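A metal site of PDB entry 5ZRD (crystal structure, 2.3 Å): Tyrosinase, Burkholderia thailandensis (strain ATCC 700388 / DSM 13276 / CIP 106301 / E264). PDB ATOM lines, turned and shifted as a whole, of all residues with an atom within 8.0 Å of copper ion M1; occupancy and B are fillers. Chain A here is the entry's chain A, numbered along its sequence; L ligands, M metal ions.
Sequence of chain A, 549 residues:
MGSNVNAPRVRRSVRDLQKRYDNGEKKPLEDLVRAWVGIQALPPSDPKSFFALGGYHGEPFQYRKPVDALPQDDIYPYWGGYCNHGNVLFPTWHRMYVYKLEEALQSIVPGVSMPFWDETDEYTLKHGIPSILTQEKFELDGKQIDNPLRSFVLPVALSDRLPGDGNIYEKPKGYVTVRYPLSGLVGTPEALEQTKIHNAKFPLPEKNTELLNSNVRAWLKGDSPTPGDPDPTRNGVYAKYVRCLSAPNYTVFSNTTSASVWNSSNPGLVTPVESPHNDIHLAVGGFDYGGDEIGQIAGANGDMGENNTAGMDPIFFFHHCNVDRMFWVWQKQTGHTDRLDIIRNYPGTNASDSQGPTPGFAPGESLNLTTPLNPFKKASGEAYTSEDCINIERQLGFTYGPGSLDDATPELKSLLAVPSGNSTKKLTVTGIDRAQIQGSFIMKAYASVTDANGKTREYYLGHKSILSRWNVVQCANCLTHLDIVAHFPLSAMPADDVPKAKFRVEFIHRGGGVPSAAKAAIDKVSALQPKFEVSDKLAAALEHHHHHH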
ATOM      1  N   HIS A  57     -20.790  27.126  25.604  1.00  0.00           N
ATOM      2  CA  HIS A  57     -19.410  26.799  25.354  1.00  0.00           C
ATOM      3  C   HIS A  57     -18.898  27.561  24.128  1.00  0.00           C
ATOM      4  O   HIS A  57     -17.917  28.308  24.203  1.00  0.00           O
ATOM      5  CB  HIS A  57     -19.265  25.286  25.134  1.00  0.00           C
ATOM      6  CG  HIS A  57     -17.855  24.834  25.158  1.00  0.00           C
ATOM      7  ND1 HIS A  57     -17.159  24.550  24.014  1.00  0.00           N
ATOM      8  CD2 HIS A  57     -16.983  24.695  26.189  1.00  0.00           C
ATOM      9  CE1 HIS A  57     -15.934  24.204  24.336  1.00  0.00           C
ATOM     10  NE2 HIS A  57     -15.795  24.317  25.664  1.00  0.00           N
ATOM     11  N   GLY A  58     -19.603  27.365  23.028  1.00  0.00           N
ATOM     12  CA  GLY A  58     -19.237  27.833  21.709  1.00  0.00           C
ATOM     13  C   GLY A  58     -20.436  28.467  20.990  1.00  0.00           C
ATOM     14  O   GLY A  58     -20.891  29.544  21.361  1.00  0.00           O
ATOM     15  N   TRP A  79     -13.335  35.031  20.170  1.00  0.00           N
ATOM     16  CA  TRP A  79     -14.225  33.876  20.390  1.00  0.00           C
ATOM     17  C   TRP A  79     -15.629  34.349  20.774  1.00  0.00           C
ATOM     18  O   TRP A  79     -15.787  35.109  21.764  1.00  0.00           O
ATOM     19  CB  TRP A  79     -13.674  32.984  21.498  1.00  0.00           C
ATOM     20  CG  TRP A  79     -14.391  31.698  21.696  1.00  0.00           C
ATOM     21  CD1 TRP A  79     -14.877  31.219  22.888  1.00  0.00           C
ATOM     22  CD2 TRP A  79     -14.656  30.682  20.717  1.00  0.00           C
ATOM     23  NE1 TRP A  79     -15.450  29.992  22.707  1.00  0.00           N
ATOM     24  CE2 TRP A  79     -15.327  29.637  21.376  1.00  0.00           C
ATOM     25  CE3 TRP A  79     -14.405  30.541  19.354  1.00  0.00           C
ATOM     26  CZ2 TRP A  79     -15.716  28.460  20.711  1.00  0.00           C
ATOM     27  CZ3 TRP A  79     -14.796  29.379  18.703  1.00  0.00           C
ATOM     28  CH2 TRP A  79     -15.448  28.355  19.373  1.00  0.00           C
ATOM     29  N   TYR A  82     -18.394  31.514  25.234  1.00  0.00           N
ATOM     30  CA  TYR A  82     -17.977  31.939  26.554  1.00  0.00           C
ATOM     31  C   TYR A  82     -16.764  31.123  27.057  1.00  0.00           C
ATOM     32  O   TYR A  82     -16.075  31.538  28.021  1.00  0.00           O
ATOM     33  CB  TYR A  82     -19.182  31.805  27.482  1.00  0.00           C
ATOM     34  CG  TYR A  82     -20.232  32.870  27.303  1.00  0.00           C
ATOM     35  CD1 TYR A  82     -19.916  34.202  27.563  1.00  0.00           C
ATOM     36  CD2 TYR A  82     -21.512  32.576  26.862  1.00  0.00           C
ATOM     37  CE1 TYR A  82     -20.851  35.206  27.394  1.00  0.00           C
ATOM     38  CE2 TYR A  82     -22.471  33.563  26.723  1.00  0.00           C
ATOM     39  CZ  TYR A  82     -22.142  34.876  27.006  1.00  0.00           C
ATOM     40  OH  TYR A  82     -23.043  35.885  26.854  1.00  0.00           O
ATOM     41  N   CYS A  83     -16.501  29.930  26.495  1.00  0.00           N
ATOM     42  CA  CYS A  83     -15.506  29.074  27.108  1.00  0.00           C
ATOM     43  C   CYS A  83     -14.147  29.762  26.972  1.00  0.00           C
ATOM     44  O   CYS A  83     -13.891  30.502  25.977  1.00  0.00           O
ATOM     45  CB  CYS A  83     -15.527  27.659  26.559  1.00  0.00           C
ATOM     46  SG  CYS A  83     -14.911  27.501  24.849  1.00  0.00           S
ATOM     47  N   ASN A  84     -13.323  29.565  28.013  1.00  0.00           N
ATOM     48  CA  ASN A  84     -11.935  30.030  28.079  1.00  0.00           C
ATOM     49  C   ASN A  84     -10.996  28.867  27.693  1.00  0.00           C
ATOM     50  O   ASN A  84     -11.034  27.801  28.322  1.00  0.00           O
ATOM     51  CB  ASN A  84     -11.581  30.562  29.466  1.00  0.00           C
ATOM     52  CG  ASN A  84     -12.041  31.978  29.678  1.00  0.00           C
ATOM     53  OD1 ASN A  84     -11.426  32.885  29.128  1.00  0.00           O
ATOM     54  ND2 ASN A  84     -13.130  32.171  30.406  1.00  0.00           N
ATOM     55  N   HIS A  85     -10.119  29.135  26.710  1.00  0.00           N
ATOM     56  CA  HIS A  85      -9.118  28.182  26.196  1.00  0.00           C
ATOM     57  C   HIS A  85      -7.792  28.891  25.913  1.00  0.00           C
ATOM     58  O   HIS A  85      -7.771  30.046  25.569  1.00  0.00           O
ATOM     59  CB  HIS A  85      -9.613  27.542  24.901  1.00  0.00           C
ATOM     60  CG  HIS A  85     -10.966  26.949  25.069  1.00  0.00           C
ATOM     61  ND1 HIS A  85     -12.102  27.640  24.804  1.00  0.00           N
ATOM     62  CD2 HIS A  85     -11.357  25.758  25.593  1.00  0.00           C
ATOM     63  CE1 HIS A  85     -13.134  26.879  25.091  1.00  0.00           C
ATOM     64  NE2 HIS A  85     -12.715  25.717  25.578  1.00  0.00           N
ATOM     65  N   PHE A  90      -8.867  28.635  31.912  1.00  0.00           N
ATOM     66  CA  PHE A  90      -9.373  27.357  31.368  1.00  0.00           C
ATOM     67  C   PHE A  90      -9.930  26.451  32.504  1.00  0.00           C
ATOM     68  O   PHE A  90     -11.034  25.938  32.406  1.00  0.00           O
ATOM     69  CB  PHE A  90      -8.312  26.677  30.493  1.00  0.00           C
ATOM     70  CG  PHE A  90      -8.609  25.223  30.235  1.00  0.00           C
ATOM     71  CD1 PHE A  90      -9.418  24.835  29.191  1.00  0.00           C
ATOM     72  CD2 PHE A  90      -8.152  24.241  31.097  1.00  0.00           C
ATOM     73  CE1 PHE A  90      -9.726  23.497  28.984  1.00  0.00           C
ATOM     74  CE2 PHE A  90      -8.438  22.909  30.887  1.00  0.00           C
ATOM     75  CZ  PHE A  90      -9.231  22.534  29.818  1.00  0.00           C
ATOM     76  N   TRP A  93     -13.002  28.134  34.611  1.00  0.00           N
ATOM     77  CA  TRP A  93     -14.200  28.374  33.814  1.00  0.00           C
ATOM     78  C   TRP A  93     -14.912  27.056  33.633  1.00  0.00           C
ATOM     79  O   TRP A  93     -16.142  27.020  33.797  1.00  0.00           O
ATOM     80  CB  TRP A  93     -13.912  29.030  32.471  1.00  0.00           C
ATOM     81  CG  TRP A  93     -15.175  29.384  31.746  1.00  0.00           C
ATOM     82  CD1 TRP A  93     -15.868  30.556  31.869  1.00  0.00           C
ATOM     83  CD2 TRP A  93     -15.931  28.537  30.868  1.00  0.00           C
ATOM     84  NE1 TRP A  93     -16.990  30.506  31.087  1.00  0.00           N
ATOM     85  CE2 TRP A  93     -17.076  29.272  30.480  1.00  0.00           C
ATOM     86  CE3 TRP A  93     -15.771  27.238  30.374  1.00  0.00           C
ATOM     87  CZ2 TRP A  93     -18.038  28.763  29.630  1.00  0.00           C
ATOM     88  CZ3 TRP A  93     -16.728  26.731  29.537  1.00  0.00           C
ATOM     89  CH2 TRP A  93     -17.840  27.488  29.161  1.00  0.00           C
ATOM     90  N   HIS A  94     -14.164  26.012  33.247  1.00  0.00           N
ATOM     91  CA  HIS A  94     -14.798  24.724  33.003  1.00  0.00           C
ATOM     92  C   HIS A  94     -15.301  24.140  34.319  1.00  0.00           C
ATOM     93  O   HIS A  94     -16.268  23.433  34.292  1.00  0.00           O
ATOM     94  CB  HIS A  94     -13.904  23.739  32.266  1.00  0.00           C
ATOM     95  CG  HIS A  94     -13.710  24.149  30.861  1.00  0.00           C
ATOM     96  ND1 HIS A  94     -12.857  25.141  30.544  1.00  0.00           N
ATOM     97  CD2 HIS A  94     -14.299  23.761  29.707  1.00  0.00           C
ATOM     98  CE1 HIS A  94     -12.916  25.360  29.242  1.00  0.00           C
ATOM     99  NE2 HIS A  94     -13.778  24.499  28.702  1.00  0.00           N
ATOM    100  N   TYR A  97     -18.559  25.582  34.605  1.00  0.00           N
ATOM    101  CA  TYR A  97     -19.432  25.104  33.530  1.00  0.00           C
ATOM    102  C   TYR A  97     -20.044  23.772  33.945  1.00  0.00           C
ATOM    103  O   TYR A  97     -21.259  23.579  33.808  1.00  0.00           O
ATOM    104  CB  TYR A  97     -18.672  24.966  32.208  1.00  0.00           C
ATOM    105  CG  TYR A  97     -19.483  24.700  30.958  1.00  0.00           C
ATOM    106  CD1 TYR A  97     -20.833  25.001  30.856  1.00  0.00           C
ATOM    107  CD2 TYR A  97     -18.864  24.177  29.837  1.00  0.00           C
ATOM    108  CE1 TYR A  97     -21.550  24.794  29.677  1.00  0.00           C
ATOM    109  CE2 TYR A  97     -19.546  24.010  28.651  1.00  0.00           C
ATOM    110  CZ  TYR A  97     -20.891  24.304  28.571  1.00  0.00           C
ATOM    111  OH  TYR A  97     -21.552  24.090  27.410  1.00  0.00           O
ATOM    112  N   GLU A 274      -4.620  21.257  30.244  1.00  0.00           N
ATOM    113  CA  GLU A 274      -5.308  21.549  28.990  1.00  0.00           C
ATOM    114  C   GLU A 274      -4.852  20.621  27.848  1.00  0.00           C
ATOM    115  O   GLU A 274      -5.611  20.415  26.899  1.00  0.00           O
ATOM    116  CB  GLU A 274      -5.114  23.003  28.561  1.00  0.00           C
ATOM    117  CG  GLU A 274      -6.151  23.472  27.574  1.00  0.00           C
ATOM    118  CD  GLU A 274      -6.054  24.922  27.133  1.00  0.00           C
ATOM    119  OE1 GLU A 274      -6.986  25.404  26.388  1.00  0.00           O
ATOM    120  OE2 GLU A 274      -5.007  25.561  27.471  1.00  0.00           O
ATOM    121  N   HIS A 277      -6.296  17.027  27.926  1.00  0.00           N
ATOM    122  CA  HIS A 277      -7.696  17.423  27.667  1.00  0.00           C
ATOM    123  C   HIS A 277      -7.940  17.558  26.156  1.00  0.00           C
ATOM    124  O   HIS A 277      -8.843  16.941  25.627  1.00  0.00           O
ATOM    125  CB  HIS A 277      -8.073  18.690  28.425  1.00  0.00           C
ATOM    126  CG  HIS A 277      -9.065  19.553  27.732  1.00  0.00           C
ATOM    127  ND1 HIS A 277      -8.693  20.479  26.764  1.00  0.00           N
ATOM    128  CD2 HIS A 277     -10.400  19.680  27.865  1.00  0.00           C
ATOM    129  CE1 HIS A 277      -9.763  21.129  26.331  1.00  0.00           C
ATOM    130  NE2 HIS A 277     -10.820  20.678  26.992  1.00  0.00           N
ATOM    131  N   ASN A 278      -7.132  18.387  25.518  1.00  0.00           N
ATOM    132  CA  ASN A 278      -7.135  18.542  24.073  1.00  0.00           C
ATOM    133  C   ASN A 278      -7.118  17.168  23.381  1.00  0.00           C
ATOM    134  O   ASN A 278      -7.921  16.930  22.458  1.00  0.00           O
ATOM    135  CB  ASN A 278      -5.988  19.432  23.606  1.00  0.00           C
ATOM    136  CG  ASN A 278      -6.205  20.891  23.916  1.00  0.00           C
ATOM    137  OD1 ASN A 278      -7.203  21.263  24.527  1.00  0.00           O
ATOM    138  ND2 ASN A 278      -5.262  21.736  23.507  1.00  0.00           N
ATOM    139  N   HIS A 281     -10.577  15.324  23.421  1.00  0.00           N
ATOM    140  CA  HIS A 281     -11.415  15.941  22.442  1.00  0.00           C
ATOM    141  C   HIS A 281     -11.061  15.439  21.029  1.00  0.00           C
ATOM    142  O   HIS A 281     -11.947  15.186  20.271  1.00  0.00           O
ATOM    143  CB  HIS A 281     -11.232  17.461  22.490  1.00  0.00           C
ATOM    144  CG  HIS A 281     -12.087  18.159  23.485  1.00  0.00           C
ATOM    145  ND1 HIS A 281     -13.265  18.776  23.129  1.00  0.00           N
ATOM    146  CD2 HIS A 281     -11.903  18.412  24.802  1.00  0.00           C
ATOM    147  CE1 HIS A 281     -13.767  19.390  24.188  1.00  0.00           C
ATOM    148  NE2 HIS A 281     -12.970  19.131  25.247  1.00  0.00           N
ATOM    149  N   GLU A 306     -13.653  20.117  17.819  1.00  0.00           N
ATOM    150  CA  GLU A 306     -13.422  21.541  17.743  1.00  0.00           C
ATOM    151  C   GLU A 306     -14.307  22.214  18.818  1.00  0.00           C
ATOM    152  O   GLU A 306     -15.249  21.599  19.364  1.00  0.00           O
ATOM    153  CB  GLU A 306     -13.804  22.111  16.375  1.00  0.00           C
ATOM    154  CG  GLU A 306     -12.735  21.951  15.280  1.00  0.00           C
ATOM    155  CD  GLU A 306     -12.494  20.568  14.683  1.00  0.00           C
ATOM    156  OE1 GLU A 306     -13.332  19.672  14.839  1.00  0.00           O
ATOM    157  OE2 GLU A 306     -11.431  20.394  14.048  1.00  0.00           O
ATOM    158  N   ASN A 307     -14.017  23.455  19.157  1.00  0.00           N
ATOM    159  CA  ASN A 307     -14.683  24.049  20.283  1.00  0.00           C
ATOM    160  C   ASN A 307     -16.101  24.494  19.864  1.00  0.00           C
ATOM    161  O   ASN A 307     -16.940  24.769  20.726  1.00  0.00           O
ATOM    162  CB  ASN A 307     -13.846  25.171  20.862  1.00  0.00           C
ATOM    163  CG  ASN A 307     -12.749  24.670  21.776  1.00  0.00           C
ATOM    164  OD1 ASN A 307     -11.654  25.241  21.810  1.00  0.00           O
ATOM    165  ND2 ASN A 307     -13.015  23.599  22.519  1.00  0.00           N
ATOM    166  N   ALA A 310     -18.667  21.220  20.467  1.00  0.00           N
ATOM    167  CA  ALA A 310     -18.340  20.114  21.397  1.00  0.00           C
ATOM    168  C   ALA A 310     -19.278  20.099  22.601  1.00  0.00           C
ATOM    169  O   ALA A 310     -19.580  19.058  23.156  1.00  0.00           O
ATOM    170  CB  ALA A 310     -16.931  20.279  21.881  1.00  0.00           C
ATOM    171  N   GLY A 311     -19.698  21.271  23.054  1.00  0.00           N
ATOM    172  CA  GLY A 311     -20.574  21.331  24.246  1.00  0.00           C
ATOM    173  C   GLY A 311     -21.939  20.687  24.006  1.00  0.00           C
ATOM    174  O   GLY A 311     -22.651  20.445  24.975  1.00  0.00           O
ATOM    175  N   PHE A 316     -19.043  15.566  26.486  1.00  0.00           N
ATOM    176  CA  PHE A 316     -18.276  16.754  26.908  1.00  0.00           C
ATOM    177  C   PHE A 316     -18.234  16.883  28.438  1.00  0.00           C
ATOM    178  O   PHE A 316     -17.194  17.148  28.987  1.00  0.00           O
ATOM    179  CB  PHE A 316     -18.859  18.026  26.317  1.00  0.00           C
ATOM    180  CG  PHE A 316     -18.113  19.278  26.710  1.00  0.00           C
ATOM    181  CD1 PHE A 316     -18.383  19.908  27.910  1.00  0.00           C
ATOM    182  CD2 PHE A 316     -17.166  19.829  25.863  1.00  0.00           C
ATOM    183  CE1 PHE A 316     -17.704  21.059  28.252  1.00  0.00           C
ATOM    184  CE2 PHE A 316     -16.467  20.976  26.212  1.00  0.00           C
ATOM    185  CZ  PHE A 316     -16.735  21.583  27.409  1.00  0.00           C
ATOM    186  N   HIS A 320     -15.085  16.588  30.989  1.00  0.00           N
ATOM    187  CA  HIS A 320     -14.718  17.764  31.709  1.00  0.00           C
ATOM    188  C   HIS A 320     -14.893  17.599  33.209  1.00  0.00           C
ATOM    189  O   HIS A 320     -14.226  18.319  33.942  1.00  0.00           O
ATOM    190  CB  HIS A 320     -15.459  19.003  31.201  1.00  0.00           C
ATOM    191  CG  HIS A 320     -14.628  19.749  30.227  1.00  0.00           C
ATOM    192  ND1 HIS A 320     -13.611  20.577  30.622  1.00  0.00           N
ATOM    193  CD2 HIS A 320     -14.613  19.748  28.879  1.00  0.00           C
ATOM    194  CE1 HIS A 320     -13.014  21.063  29.561  1.00  0.00           C
ATOM    195  NE2 HIS A 320     -13.623  20.597  28.488  1.00  0.00           N
ATOM    196  N   GLN A 355      -7.345  31.921  21.489  1.00  0.00           N
ATOM    197  CA  GLN A 355      -8.671  32.049  20.849  1.00  0.00           C
ATOM    198  C   GLN A 355      -9.110  33.508  20.706  1.00  0.00           C
ATOM    199  O   GLN A 355      -9.982  33.812  19.896  1.00  0.00           O
ATOM    200  CB  GLN A 355      -9.713  31.299  21.688  1.00  0.00           C
ATOM    201  CG  GLN A 355     -10.044  31.958  23.025  1.00  0.00           C
ATOM    202  CD  GLN A 355     -11.070  31.188  23.798  1.00  0.00           C
ATOM    203  OE1 GLN A 355     -11.538  30.105  23.390  1.00  0.00           O
ATOM    204  NE2 GLN A 355     -11.408  31.735  24.943  1.00  0.00           N
ATOM    205  N   LEU A 467      -6.357  21.833  19.928  1.00  0.00           N
ATOM    206  CA  LEU A 467      -7.809  21.928  19.868  1.00  0.00           C
ATOM    207  C   LEU A 467      -8.147  23.335  19.441  1.00  0.00           C
ATOM    208  O   LEU A 467      -7.787  24.270  20.140  1.00  0.00           O
ATOM    209  CB  LEU A 467      -8.393  21.669  21.249  1.00  0.00           C
ATOM    210  CG  LEU A 467      -9.905  21.780  21.383  1.00  0.00           C
ATOM    211  CD1 LEU A 467     -10.603  20.751  20.504  1.00  0.00           C
ATOM    212  CD2 LEU A 467     -10.309  21.584  22.847  1.00  0.00           C
HETATM  213  O1  LIG L   1     -12.762  22.391  25.848  1.00  0.00           O
HETATM  214 CU    CU M   1     -14.004  24.413  26.558  1.00  0.00          CU
HETATM  215 CU    CU M   2     -12.928  20.433  26.768  1.00  0.00          CU
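The backbone carbonyl oxygen (O) of His 57 is in hydrogen-bond range of the backbone NH (N) of Cys 83 (3.1 Å).
The backbone carbonyl oxygen (O) of Phe 90 lies within hydrogen-bond range of a ring nitrogen (ND1) of His 94 (2.7 Å).
O of His 57 is in hydrogen-bond range of NE1 of Trp 79, at 3.3 Å.
The backbone carbonyl oxygen of Asn 307 lies within hydrogen-bond range of a ring nitrogen (ND1) of His 57.
O of His 57 lies within hydrogen-bond range of N of Tyr 82 (3.4 Å).
The side-chain sulfur (SG) of Cys 83 sits at hydrogen-bond distance from the indole nitrogen (NE1) of Trp 79.
O of Cys 83 sits at hydrogen-bond distance from NE2 of Gln 355, 3.0 Å away.
OE1 of Gln 355 sits at hydrogen-bond distance from ND1 of His 85, at 2.9 Å.
Copper ion M1 is bound by a ring nitrogen (NE2) of His 57, a ring nitrogen (NE2) of His 85, a ring nitrogen (NE2) of His 94 and an oxygen (O1) of the ligand.
Residues that only touch copper ion M1: Cys 83 (3.6 Å).
Of the 23 residues printed, 4 come within 4 Å of copper ion M1.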
